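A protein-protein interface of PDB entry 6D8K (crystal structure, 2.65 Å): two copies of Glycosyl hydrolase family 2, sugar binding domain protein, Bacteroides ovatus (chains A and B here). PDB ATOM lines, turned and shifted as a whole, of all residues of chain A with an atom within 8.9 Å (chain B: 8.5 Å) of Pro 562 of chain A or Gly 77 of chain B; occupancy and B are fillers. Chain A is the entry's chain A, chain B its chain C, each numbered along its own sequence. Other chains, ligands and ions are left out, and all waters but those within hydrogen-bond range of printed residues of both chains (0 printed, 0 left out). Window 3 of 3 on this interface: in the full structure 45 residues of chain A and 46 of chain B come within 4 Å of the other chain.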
ATOM      1  N   LEU A 508      28.445  15.116  10.889  1.00  0.00           N
ATOM      2  CA  LEU A 508      28.282  13.875  11.625  1.00  0.00           C
ATOM      3  C   LEU A 508      28.648  12.730  10.694  1.00  0.00           C
ATOM      4  O   LEU A 508      28.131  12.646   9.577  1.00  0.00           O
ATOM      5  CB  LEU A 508      26.846  13.741  12.129  1.00  0.00           C
ATOM      6  CG  LEU A 508      26.541  12.500  12.982  1.00  0.00           C
ATOM      7  CD1 LEU A 508      27.244  12.627  14.317  1.00  0.00           C
ATOM      8  CD2 LEU A 508      25.032  12.278  13.212  1.00  0.00           C
ATOM      9  N   TRP A 521      24.647  19.021   8.223  1.00  0.00           N
ATOM     10  CA  TRP A 521      25.662  18.279   8.978  1.00  0.00           C
ATOM     11  C   TRP A 521      26.025  16.987   8.259  1.00  0.00           C
ATOM     12  O   TRP A 521      26.261  15.948   8.879  1.00  0.00           O
ATOM     13  CB  TRP A 521      25.203  17.984  10.415  1.00  0.00           C
ATOM     14  CG  TRP A 521      25.885  18.831  11.465  1.00  0.00           C
ATOM     15  CD1 TRP A 521      26.994  18.501  12.195  1.00  0.00           C
ATOM     16  CD2 TRP A 521      25.501  20.139  11.896  1.00  0.00           C
ATOM     17  NE1 TRP A 521      27.326  19.526  13.048  1.00  0.00           N
ATOM     18  CE2 TRP A 521      26.432  20.547  12.885  1.00  0.00           C
ATOM     19  CE3 TRP A 521      24.470  21.018  11.531  1.00  0.00           C
ATOM     20  CZ2 TRP A 521      26.364  21.788  13.513  1.00  0.00           C
ATOM     21  CZ3 TRP A 521      24.398  22.248  12.157  1.00  0.00           C
ATOM     22  CH2 TRP A 521      25.336  22.620  13.147  1.00  0.00           C
ATOM     23  N   ARG A 559      28.537  23.300  22.048  1.00  0.00           N
ATOM     24  CA  ARG A 559      28.027  22.685  20.827  1.00  0.00           C
ATOM     25  C   ARG A 559      26.822  21.859  21.247  1.00  0.00           C
ATOM     26  O   ARG A 559      26.946  20.668  21.558  1.00  0.00           O
ATOM     27  CB  ARG A 559      29.096  21.828  20.168  1.00  0.00           C
ATOM     28  CG  ARG A 559      30.460  22.490  20.112  1.00  0.00           C
ATOM     29  CD  ARG A 559      30.464  23.587  19.103  1.00  0.00           C
ATOM     30  NE  ARG A 559      31.710  24.354  19.113  1.00  0.00           N
ATOM     31  CZ  ARG A 559      32.029  25.232  18.169  1.00  0.00           C
ATOM     32  NH1 ARG A 559      31.212  25.414  17.151  1.00  0.00           N
ATOM     33  NH2 ARG A 559      33.147  25.918  18.235  1.00  0.00           N
ATOM     34  N   PHE A 560      25.645  22.508  21.250  1.00  0.00           N
ATOM     35  CA  PHE A 560      24.436  22.009  21.894  1.00  0.00           C
ATOM     36  C   PHE A 560      23.489  21.274  20.980  1.00  0.00           C
ATOM     37  O   PHE A 560      22.430  20.853  21.461  1.00  0.00           O
ATOM     38  CB  PHE A 560      23.580  23.132  22.470  1.00  0.00           C
ATOM     39  CG  PHE A 560      24.313  24.143  23.250  1.00  0.00           C
ATOM     40  CD1 PHE A 560      24.871  23.828  24.461  1.00  0.00           C
ATOM     41  CD2 PHE A 560      24.385  25.432  22.802  1.00  0.00           C
ATOM     42  CE1 PHE A 560      25.504  24.782  25.197  1.00  0.00           C
ATOM     43  CE2 PHE A 560      25.035  26.381  23.522  1.00  0.00           C
ATOM     44  CZ  PHE A 560      25.592  26.067  24.719  1.00  0.00           C
ATOM     45  N   HIS A 561      23.746  21.211  19.680  1.00  0.00           N
ATOM     46  CA  HIS A 561      22.692  20.667  18.839  1.00  0.00           C
ATOM     47  C   HIS A 561      22.466  19.236  19.271  1.00  0.00           C
ATOM     48  O   HIS A 561      23.420  18.454  19.284  1.00  0.00           O
ATOM     49  CB  HIS A 561      23.038  20.718  17.374  1.00  0.00           C
ATOM     50  CG  HIS A 561      21.870  20.460  16.495  1.00  0.00           C
ATOM     51  ND1 HIS A 561      21.379  19.194  16.270  1.00  0.00           N
ATOM     52  CD2 HIS A 561      21.067  21.305  15.806  1.00  0.00           C
ATOM     53  CE1 HIS A 561      20.340  19.263  15.459  1.00  0.00           C
ATOM     54  NE2 HIS A 561      20.123  20.534  15.171  1.00  0.00           N
ATOM     55  N   PRO A 562      21.259  18.864  19.683  1.00  0.00           N
ATOM     56  CA  PRO A 562      21.115  17.572  20.355  1.00  0.00           C
ATOM     57  C   PRO A 562      21.443  16.407  19.458  1.00  0.00           C
ATOM     58  O   PRO A 562      22.063  15.432  19.908  1.00  0.00           O
ATOM     59  CB  PRO A 562      19.646  17.587  20.800  1.00  0.00           C
ATOM     60  CG  PRO A 562      19.317  19.038  20.910  1.00  0.00           C
ATOM     61  CD  PRO A 562      20.007  19.634  19.735  1.00  0.00           C
ATOM     62  N   THR A 563      21.069  16.492  18.183  1.00  0.00           N
ATOM     63  CA  THR A 563      21.208  15.362  17.277  1.00  0.00           C
ATOM     64  C   THR A 563      22.415  15.456  16.350  1.00  0.00           C
ATOM     65  O   THR A 563      22.901  14.416  15.901  1.00  0.00           O
ATOM     66  CB  THR A 563      19.933  15.197  16.447  1.00  0.00           C
ATOM     67  OG1 THR A 563      19.655  16.415  15.754  1.00  0.00           O
ATOM     68  CG2 THR A 563      18.767  14.849  17.339  1.00  0.00           C
ATOM     69  N   ASN A 564      22.938  16.648  16.074  1.00  0.00           N
ATOM     70  CA  ASN A 564      24.140  16.746  15.246  1.00  0.00           C
ATOM     71  C   ASN A 564      25.403  17.023  16.046  1.00  0.00           C
ATOM     72  O   ASN A 564      26.499  16.835  15.514  1.00  0.00           O
ATOM     73  CB  ASN A 564      24.030  17.850  14.176  1.00  0.00           C
ATOM     74  CG  ASN A 564      22.803  17.725  13.283  1.00  0.00           C
ATOM     75  OD1 ASN A 564      22.238  16.647  13.085  1.00  0.00           O
ATOM     76  ND2 ASN A 564      22.381  18.855  12.743  1.00  0.00           N
ATOM     77  N   GLN A 565      25.294  17.470  17.301  1.00  0.00           N
ATOM     78  CA  GLN A 565      26.491  17.839  18.055  1.00  0.00           C
ATOM     79  C   GLN A 565      26.644  17.052  19.350  1.00  0.00           C
ATOM     80  O   GLN A 565      27.665  16.365  19.525  1.00  0.00           O
ATOM     81  CB  GLN A 565      26.483  19.349  18.320  1.00  0.00           C
ATOM     82  CG  GLN A 565      26.748  20.207  17.072  1.00  0.00           C
ATOM     83  CD  GLN A 565      26.894  21.675  17.415  1.00  0.00           C
ATOM     84  OE1 GLN A 565      26.011  22.276  18.033  1.00  0.00           O
ATOM     85  NE2 GLN A 565      28.006  22.254  17.041  1.00  0.00           N
ATOM     86  N   ASP A 566      25.664  17.132  20.262  1.00  0.00           N
ATOM     87  CA  ASP A 566      25.691  16.385  21.519  1.00  0.00           C
ATOM     88  C   ASP A 566      27.013  16.583  22.271  1.00  0.00           C
ATOM     89  O   ASP A 566      27.619  15.633  22.770  1.00  0.00           O
ATOM     90  CB  ASP A 566      25.433  14.897  21.260  1.00  0.00           C
ATOM     91  CG  ASP A 566      25.053  14.140  22.518  1.00  0.00           C
ATOM     92  OD1 ASP A 566      24.702  14.800  23.518  1.00  0.00           O
ATOM     93  OD2 ASP A 566      25.102  12.891  22.519  1.00  0.00           O
ATOM     94  N   GLY A 567      27.494  17.819  22.311  1.00  0.00           N
ATOM     95  CA  GLY A 567      28.738  18.107  22.980  1.00  0.00           C
ATOM     96  C   GLY A 567      29.981  18.016  22.128  1.00  0.00           C
ATOM     97  O   GLY A 567      31.075  18.270  22.644  1.00  0.00           O
ATOM     98  N   TRP A 568      29.853  17.674  20.847  1.00  0.00           N
ATOM     99  CA  TRP A 568      30.981  17.543  19.931  1.00  0.00           C
ATOM    100  C   TRP A 568      31.022  18.694  18.933  1.00  0.00           C
ATOM    101  O   TRP A 568      30.025  19.002  18.274  1.00  0.00           O
ATOM    102  CB  TRP A 568      30.923  16.234  19.133  1.00  0.00           C
ATOM    103  CG  TRP A 568      30.914  14.982  19.942  1.00  0.00           C
ATOM    104  CD1 TRP A 568      29.818  14.286  20.355  1.00  0.00           C
ATOM    105  CD2 TRP A 568      32.050  14.258  20.404  1.00  0.00           C
ATOM    106  NE1 TRP A 568      30.200  13.172  21.062  1.00  0.00           N
ATOM    107  CE2 TRP A 568      31.570  13.130  21.107  1.00  0.00           C
ATOM    108  CE3 TRP A 568      33.432  14.447  20.292  1.00  0.00           C
ATOM    109  CZ2 TRP A 568      32.426  12.196  21.708  1.00  0.00           C
ATOM    110  CZ3 TRP A 568      34.286  13.521  20.896  1.00  0.00           C
ATOM    111  CH2 TRP A 568      33.773  12.408  21.593  1.00  0.00           C
ATOM    112  N   ARG A 570      31.904  18.877  15.583  1.00  0.00           N
ATOM    113  CA  ARG A 570      32.052  17.857  14.550  1.00  0.00           C
ATOM    114  C   ARG A 570      32.923  18.308  13.379  1.00  0.00           C
ATOM    115  O   ARG A 570      32.705  17.884  12.238  1.00  0.00           O
ATOM    116  CB  ARG A 570      30.683  17.453  14.023  1.00  0.00           C
ATOM    117  CG  ARG A 570      29.782  16.877  15.040  1.00  0.00           C
ATOM    118  CD  ARG A 570      30.046  15.422  15.292  1.00  0.00           C
ATOM    119  NE  ARG A 570      29.032  14.927  16.205  1.00  0.00           N
ATOM    120  CZ  ARG A 570      29.132  13.831  16.949  1.00  0.00           C
ATOM    121  NH1 ARG A 570      30.223  13.080  16.889  1.00  0.00           N
ATOM    122  NH2 ARG A 570      28.130  13.499  17.762  1.00  0.00           N
ATOM    123  N   TRP B  42       9.894  19.156  29.494  1.00  0.00           N
ATOM    124  CA  TRP B  42      10.450  20.327  28.834  1.00  0.00           C
ATOM    125  C   TRP B  42      11.783  19.973  28.192  1.00  0.00           C
ATOM    126  O   TRP B  42      12.594  19.242  28.769  1.00  0.00           O
ATOM    127  CB  TRP B  42      10.674  21.497  29.803  1.00  0.00           C
ATOM    128  CG  TRP B  42       9.465  22.153  30.403  1.00  0.00           C
ATOM    129  CD1 TRP B  42       8.377  21.541  30.977  1.00  0.00           C
ATOM    130  CD2 TRP B  42       9.259  23.560  30.562  1.00  0.00           C
ATOM    131  NE1 TRP B  42       7.497  22.489  31.463  1.00  0.00           N
ATOM    132  CE2 TRP B  42       8.018  23.734  31.219  1.00  0.00           C
ATOM    133  CE3 TRP B  42       9.995  24.694  30.192  1.00  0.00           C
ATOM    134  CZ2 TRP B  42       7.501  24.992  31.514  1.00  0.00           C
ATOM    135  CZ3 TRP B  42       9.478  25.947  30.484  1.00  0.00           C
ATOM    136  CH2 TRP B  42       8.241  26.085  31.145  1.00  0.00           C
ATOM    137  N   ASN B  43      12.028  20.522  27.014  1.00  0.00           N
ATOM    138  CA  ASN B  43      13.329  20.341  26.403  1.00  0.00           C
ATOM    139  C   ASN B  43      14.349  21.200  27.121  1.00  0.00           C
ATOM    140  O   ASN B  43      14.029  22.295  27.608  1.00  0.00           O
ATOM    141  CB  ASN B  43      13.253  20.686  24.926  1.00  0.00           C
ATOM    142  CG  ASN B  43      12.226  19.852  24.223  1.00  0.00           C
ATOM    143  OD1 ASN B  43      12.505  18.722  23.804  1.00  0.00           O
ATOM    144  ND2 ASN B  43      11.002  20.378  24.129  1.00  0.00           N
ATOM    145  N   ALA B  44      15.582  20.695  27.200  1.00  0.00           N
ATOM    146  CA  ALA B  44      16.599  21.358  27.995  1.00  0.00           C
ATOM    147  C   ALA B  44      17.958  21.258  27.321  1.00  0.00           C
ATOM    148  O   ALA B  44      18.246  20.327  26.553  1.00  0.00           O
ATOM    149  CB  ALA B  44      16.657  20.787  29.425  1.00  0.00           C
ATOM    150  N   ILE B  45      18.781  22.255  27.611  1.00  0.00           N
ATOM    151  CA  ILE B  45      20.149  22.343  27.133  1.00  0.00           C
ATOM    152  C   ILE B  45      21.033  22.666  28.327  1.00  0.00           C
ATOM    153  O   ILE B  45      20.811  23.674  29.007  1.00  0.00           O
ATOM    154  CB  ILE B  45      20.310  23.437  26.068  1.00  0.00           C
ATOM    155  CG1 ILE B  45      19.510  23.118  24.816  1.00  0.00           C
ATOM    156  CG2 ILE B  45      21.767  23.665  25.757  1.00  0.00           C
ATOM    157  CD1 ILE B  45      19.339  24.355  23.929  1.00  0.00           C
ATOM    158  N   TYR B  70      22.338  26.818  13.138  1.00  0.00           N
ATOM    159  CA  TYR B  70      22.264  27.117  14.564  1.00  0.00           C
ATOM    160  C   TYR B  70      22.732  25.919  15.386  1.00  0.00           C
ATOM    161  O   TYR B  70      22.276  24.791  15.175  1.00  0.00           O
ATOM    162  CB  TYR B  70      20.838  27.545  14.954  1.00  0.00           C
ATOM    163  CG  TYR B  70      20.372  28.692  14.108  1.00  0.00           C
ATOM    164  CD1 TYR B  70      20.791  29.993  14.370  1.00  0.00           C
ATOM    165  CD2 TYR B  70      19.551  28.469  13.008  1.00  0.00           C
ATOM    166  CE1 TYR B  70      20.376  31.056  13.559  1.00  0.00           C
ATOM    167  CE2 TYR B  70      19.132  29.512  12.199  1.00  0.00           C
ATOM    168  CZ  TYR B  70      19.543  30.802  12.473  1.00  0.00           C
ATOM    169  OH  TYR B  70      19.112  31.824  11.649  1.00  0.00           O
ATOM    170  N   GLU B  71      23.647  26.168  16.320  1.00  0.00           N
ATOM    171  CA  GLU B  71      24.322  25.073  17.019  1.00  0.00           C
ATOM    172  C   GLU B  71      23.589  24.653  18.276  1.00  0.00           C
ATOM    173  O   GLU B  71      24.199  24.382  19.298  1.00  0.00           O
ATOM    174  CB  GLU B  71      25.772  25.466  17.308  1.00  0.00           C
ATOM    175  CG  GLU B  71      26.542  25.822  16.005  1.00  0.00           C
ATOM    176  CD  GLU B  71      28.027  26.075  16.206  1.00  0.00           C
ATOM    177  OE1 GLU B  71      28.588  26.934  15.494  1.00  0.00           O
ATOM    178  OE2 GLU B  71      28.645  25.416  17.071  1.00  0.00           O
ATOM    179  N   TYR B  72      22.263  24.594  18.210  1.00  0.00           N
ATOM    180  CA  TYR B  72      21.415  24.289  19.350  1.00  0.00           C
ATOM    181  C   TYR B  72      20.041  23.962  18.802  1.00  0.00           C
ATOM    182  O   TYR B  72      19.753  24.194  17.631  1.00  0.00           O
ATOM    183  CB  TYR B  72      21.338  25.451  20.341  1.00  0.00           C
ATOM    184  CG  TYR B  72      20.505  26.623  19.850  1.00  0.00           C
ATOM    185  CD1 TYR B  72      21.109  27.711  19.237  1.00  0.00           C
ATOM    186  CD2 TYR B  72      19.114  26.643  20.001  1.00  0.00           C
ATOM    187  CE1 TYR B  72      20.376  28.781  18.778  1.00  0.00           C
ATOM    188  CE2 TYR B  72      18.350  27.730  19.541  1.00  0.00           C
ATOM    189  CZ  TYR B  72      18.997  28.800  18.929  1.00  0.00           C
ATOM    190  OH  TYR B  72      18.291  29.890  18.462  1.00  0.00           O
ATOM    191  N   SER B  73      19.173  23.469  19.681  1.00  0.00           N
ATOM    192  CA  SER B  73      17.787  23.200  19.330  1.00  0.00           C
ATOM    193  C   SER B  73      17.032  22.739  20.557  1.00  0.00           C
ATOM    194  O   SER B  73      17.619  22.167  21.479  1.00  0.00           O
ATOM    195  CB  SER B  73      17.675  22.132  18.247  1.00  0.00           C
ATOM    196  OG  SER B  73      16.628  21.243  18.587  1.00  0.00           O
ATOM    197  N   PHE B  74      15.731  22.962  20.572  1.00  0.00           N
ATOM    198  CA  PHE B  74      14.892  22.538  21.675  1.00  0.00           C
ATOM    199  C   PHE B  74      13.942  21.427  21.241  1.00  0.00           C
ATOM    200  O   PHE B  74      12.798  21.349  21.697  1.00  0.00           O
ATOM    201  CB  PHE B  74      14.120  23.717  22.251  1.00  0.00           C
ATOM    202  CG  PHE B  74      14.972  24.675  23.034  1.00  0.00           C
ATOM    203  CD1 PHE B  74      15.406  24.360  24.318  1.00  0.00           C
ATOM    204  CD2 PHE B  74      15.326  25.900  22.503  1.00  0.00           C
ATOM    205  CE1 PHE B  74      16.175  25.242  25.056  1.00  0.00           C
ATOM    206  CE2 PHE B  74      16.105  26.790  23.227  1.00  0.00           C
ATOM    207  CZ  PHE B  74      16.534  26.451  24.511  1.00  0.00           C
ATOM    208  N   GLN B  75      14.400  20.558  20.348  1.00  0.00           N
ATOM    209  CA  GLN B  75      13.605  19.407  19.966  1.00  0.00           C
ATOM    210  C   GLN B  75      14.511  18.195  19.877  1.00  0.00           C
ATOM    211  O   GLN B  75      15.640  18.306  19.407  1.00  0.00           O
ATOM    212  CB  GLN B  75      12.902  19.628  18.623  1.00  0.00           C
ATOM    213  CG  GLN B  75      11.592  18.829  18.462  1.00  0.00           C
ATOM    214  CD  GLN B  75      10.484  19.324  19.394  1.00  0.00           C
ATOM    215  OE1 GLN B  75      10.410  18.932  20.566  1.00  0.00           O
ATOM    216  NE2 GLN B  75       9.619  20.192  18.875  1.00  0.00           N
ATOM    217  N   GLY B  76      14.035  17.051  20.355  1.00  0.00           N
ATOM    218  CA  GLY B  76      14.731  15.811  20.100  1.00  0.00           C
ATOM    219  C   GLY B  76      15.989  15.576  20.898  1.00  0.00           C
ATOM    220  O   GLY B  76      16.823  14.759  20.487  1.00  0.00           O
ATOM    221  N   GLY B  77      16.144  16.244  22.039  1.00  0.00           N
ATOM    222  CA  GLY B  77      17.269  15.996  22.920  1.00  0.00           C
ATOM    223  C   GLY B  77      16.807  15.751  24.332  1.00  0.00           C
ATOM    224  O   GLY B  77      15.686  15.284  24.552  1.00  0.00           O
ATOM    225  N   LEU B  78      17.659  16.053  25.300  1.00  0.00           N
ATOM    226  CA  LEU B  78      17.307  15.912  26.704  1.00  0.00           C
ATOM    227  C   LEU B  78      16.000  16.636  27.027  1.00  0.00           C
ATOM    228  O   LEU B  78      15.787  17.793  26.648  1.00  0.00           O
ATOM    229  CB  LEU B  78      18.433  16.462  27.575  1.00  0.00           C
ATOM    230  CG  LEU B  78      18.121  16.577  29.067  1.00  0.00           C
ATOM    231  CD1 LEU B  78      18.142  15.218  29.701  1.00  0.00           C
ATOM    232  CD2 LEU B  78      19.097  17.519  29.767  1.00  0.00           C
ATOM    233  N   ARG B  79      15.135  15.951  27.762  1.00  0.00           N
ATOM    234  CA  ARG B  79      13.930  16.546  28.302  1.00  0.00           C
ATOM    235  C   ARG B  79      13.890  16.307  29.800  1.00  0.00           C
ATOM    236  O   ARG B  79      13.978  15.160  30.241  1.00  0.00           O
ATOM    237  CB  ARG B  79      12.689  15.952  27.649  1.00  0.00           C
ATOM    238  CG  ARG B  79      12.581  16.222  26.168  1.00  0.00           C
ATOM    239  CD  ARG B  79      11.208  15.828  25.709  1.00  0.00           C
ATOM    240  NE  ARG B  79      10.976  14.407  25.924  1.00  0.00           N
ATOM    241  CZ  ARG B  79       9.773  13.844  25.942  1.00  0.00           C
ATOM    242  NH1 ARG B  79       8.692  14.592  25.775  1.00  0.00           N
ATOM    243  NH2 ARG B  79       9.651  12.532  26.130  1.00  0.00           N
ATOM    244  N   LEU B  80      13.755  17.380  30.572  1.00  0.00           N
ATOM    245  CA  LEU B  80      13.685  17.301  32.020  1.00  0.00           C
ATOM    246  C   LEU B  80      12.243  17.432  32.515  1.00  0.00           C
ATOM    247  O   LEU B  80      11.431  18.173  31.952  1.00  0.00           O
ATOM    248  CB  LEU B  80      14.546  18.387  32.664  1.00  0.00           C
ATOM    249  CG  LEU B  80      16.067  18.416  32.446  1.00  0.00           C
ATOM    250  CD1 LEU B  80      16.696  19.692  33.083  1.00  0.00           C
ATOM    251  CD2 LEU B  80      16.730  17.149  32.955  1.00  0.00           C
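The backbone NH of Phe 560 of chain A lies within hydrogen-bond range of the backbone carbonyl oxygen of Glu 71 of chain B (3.1 Å). N of His 561 of chain A lies within hydrogen-bond range of O of Glu 71 of chain B (3.2 Å). O of Glu 71 of chain B sits close to OE1 of Gln 565 of chain A, at 3.1 Å. The guanidinium group of Arg 559 of chain A is in salt-bridge range of the side-chain carboxylate of Glu 71 of chain B, at 2.6 Å.
The backbone carbonyl oxygen of Gln 565 of chain A lies within hydrogen-bond range of the guanidinium group of Arg 570 of chain A (3.4 Å). O of His 561 of chain A lies within hydrogen-bond range of N of Asp 566 of chain A, at 2.8 Å. A ring nitrogen (ND1) of His 561 of chain A sits close to the side-chain hydroxyl (OG1) of Thr 563 of chain A, at 3.3 Å. The backbone carbonyl oxygen (O) of Arg 559 of chain A is in hydrogen-bond range of the backbone NH (N) of Gly 567 of chain A (3.0 Å). N of His 561 of chain A is in hydrogen-bond range of OE1 of Gln 565 of chain A (3.0 Å). The backbone NH of Asn 564 of chain A lies within hydrogen-bond range of a ring nitrogen (ND1) of His 561 of chain A (3.0 Å).
CD1 of Phe 560 of chain A touches CG2 of Ile 45 of chain B, 3.4 Å away. CB of Phe 560 of chain A touches CB of Tyr 72 of chain B (3.9 Å). His 561 of chain A touches Tyr 70 of chain B (CD2 to O, 3.7 Å). Tyr 72 of chain B touches His 561 of chain A. CG of Pro 562 of chain A touches O of Ser 73 of chain B (3.6 Å). Gly 77 of chain B touches Pro 562 of chain A (CA to CB, 3.6 Å). Thr 563 of chain A touches Gly 76 of chain B (CG2 to O, 3.7 Å).
Of the printed residues of chain B, Pro 562 of chain A touches Ser 73 (3.6 Å) and Gly 77 (3.6 Å). Of the printed residues of chain B, Phe 560 of chain A touches Ile 45 (3.4 Å), Glu 71 (3.1 Å) and Tyr 72 (3.9 Å). Printed residues of chain A within 4 Å of Glu 71 of chain B: Arg 559, Phe 560, His 561 and Gln 565. The nearest printed residue of chain B that does not touch Pro 562 of chain A is Gly 76 of chain B (4.01 Å). The nearest residue of chain A that does not touch Gly 77 of chain B is Thr 563 of chain A (5.6 Å). The nearest printed residue of chain A that does not touch Tyr 70 of chain B is Trp 521 of chain A (4.3 Å).
Of the 13 printed residues of chain A, 6 touch a printed residue of chain B. Hydrophobic or aromatic side chains of chain A within 4 Å of the printed part of chain B: Phe 560, His 561 and Pro 562. Of the 15 printed residues of chain B, 7 touch a printed residue of chain A. Among the printed residues, 11 pairs touch across the chains. Among the printed residues, Asp or Glu carboxylates within 4 Å of a Lys or Arg side-chain nitrogen of the other chain: Arg 559 of chain A with Glu 71 of chain B.
No position is printed for both chains. Of the 11 pairs that touch across the chains among the printed residues, none has its exchanged pair printed and touching as well.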
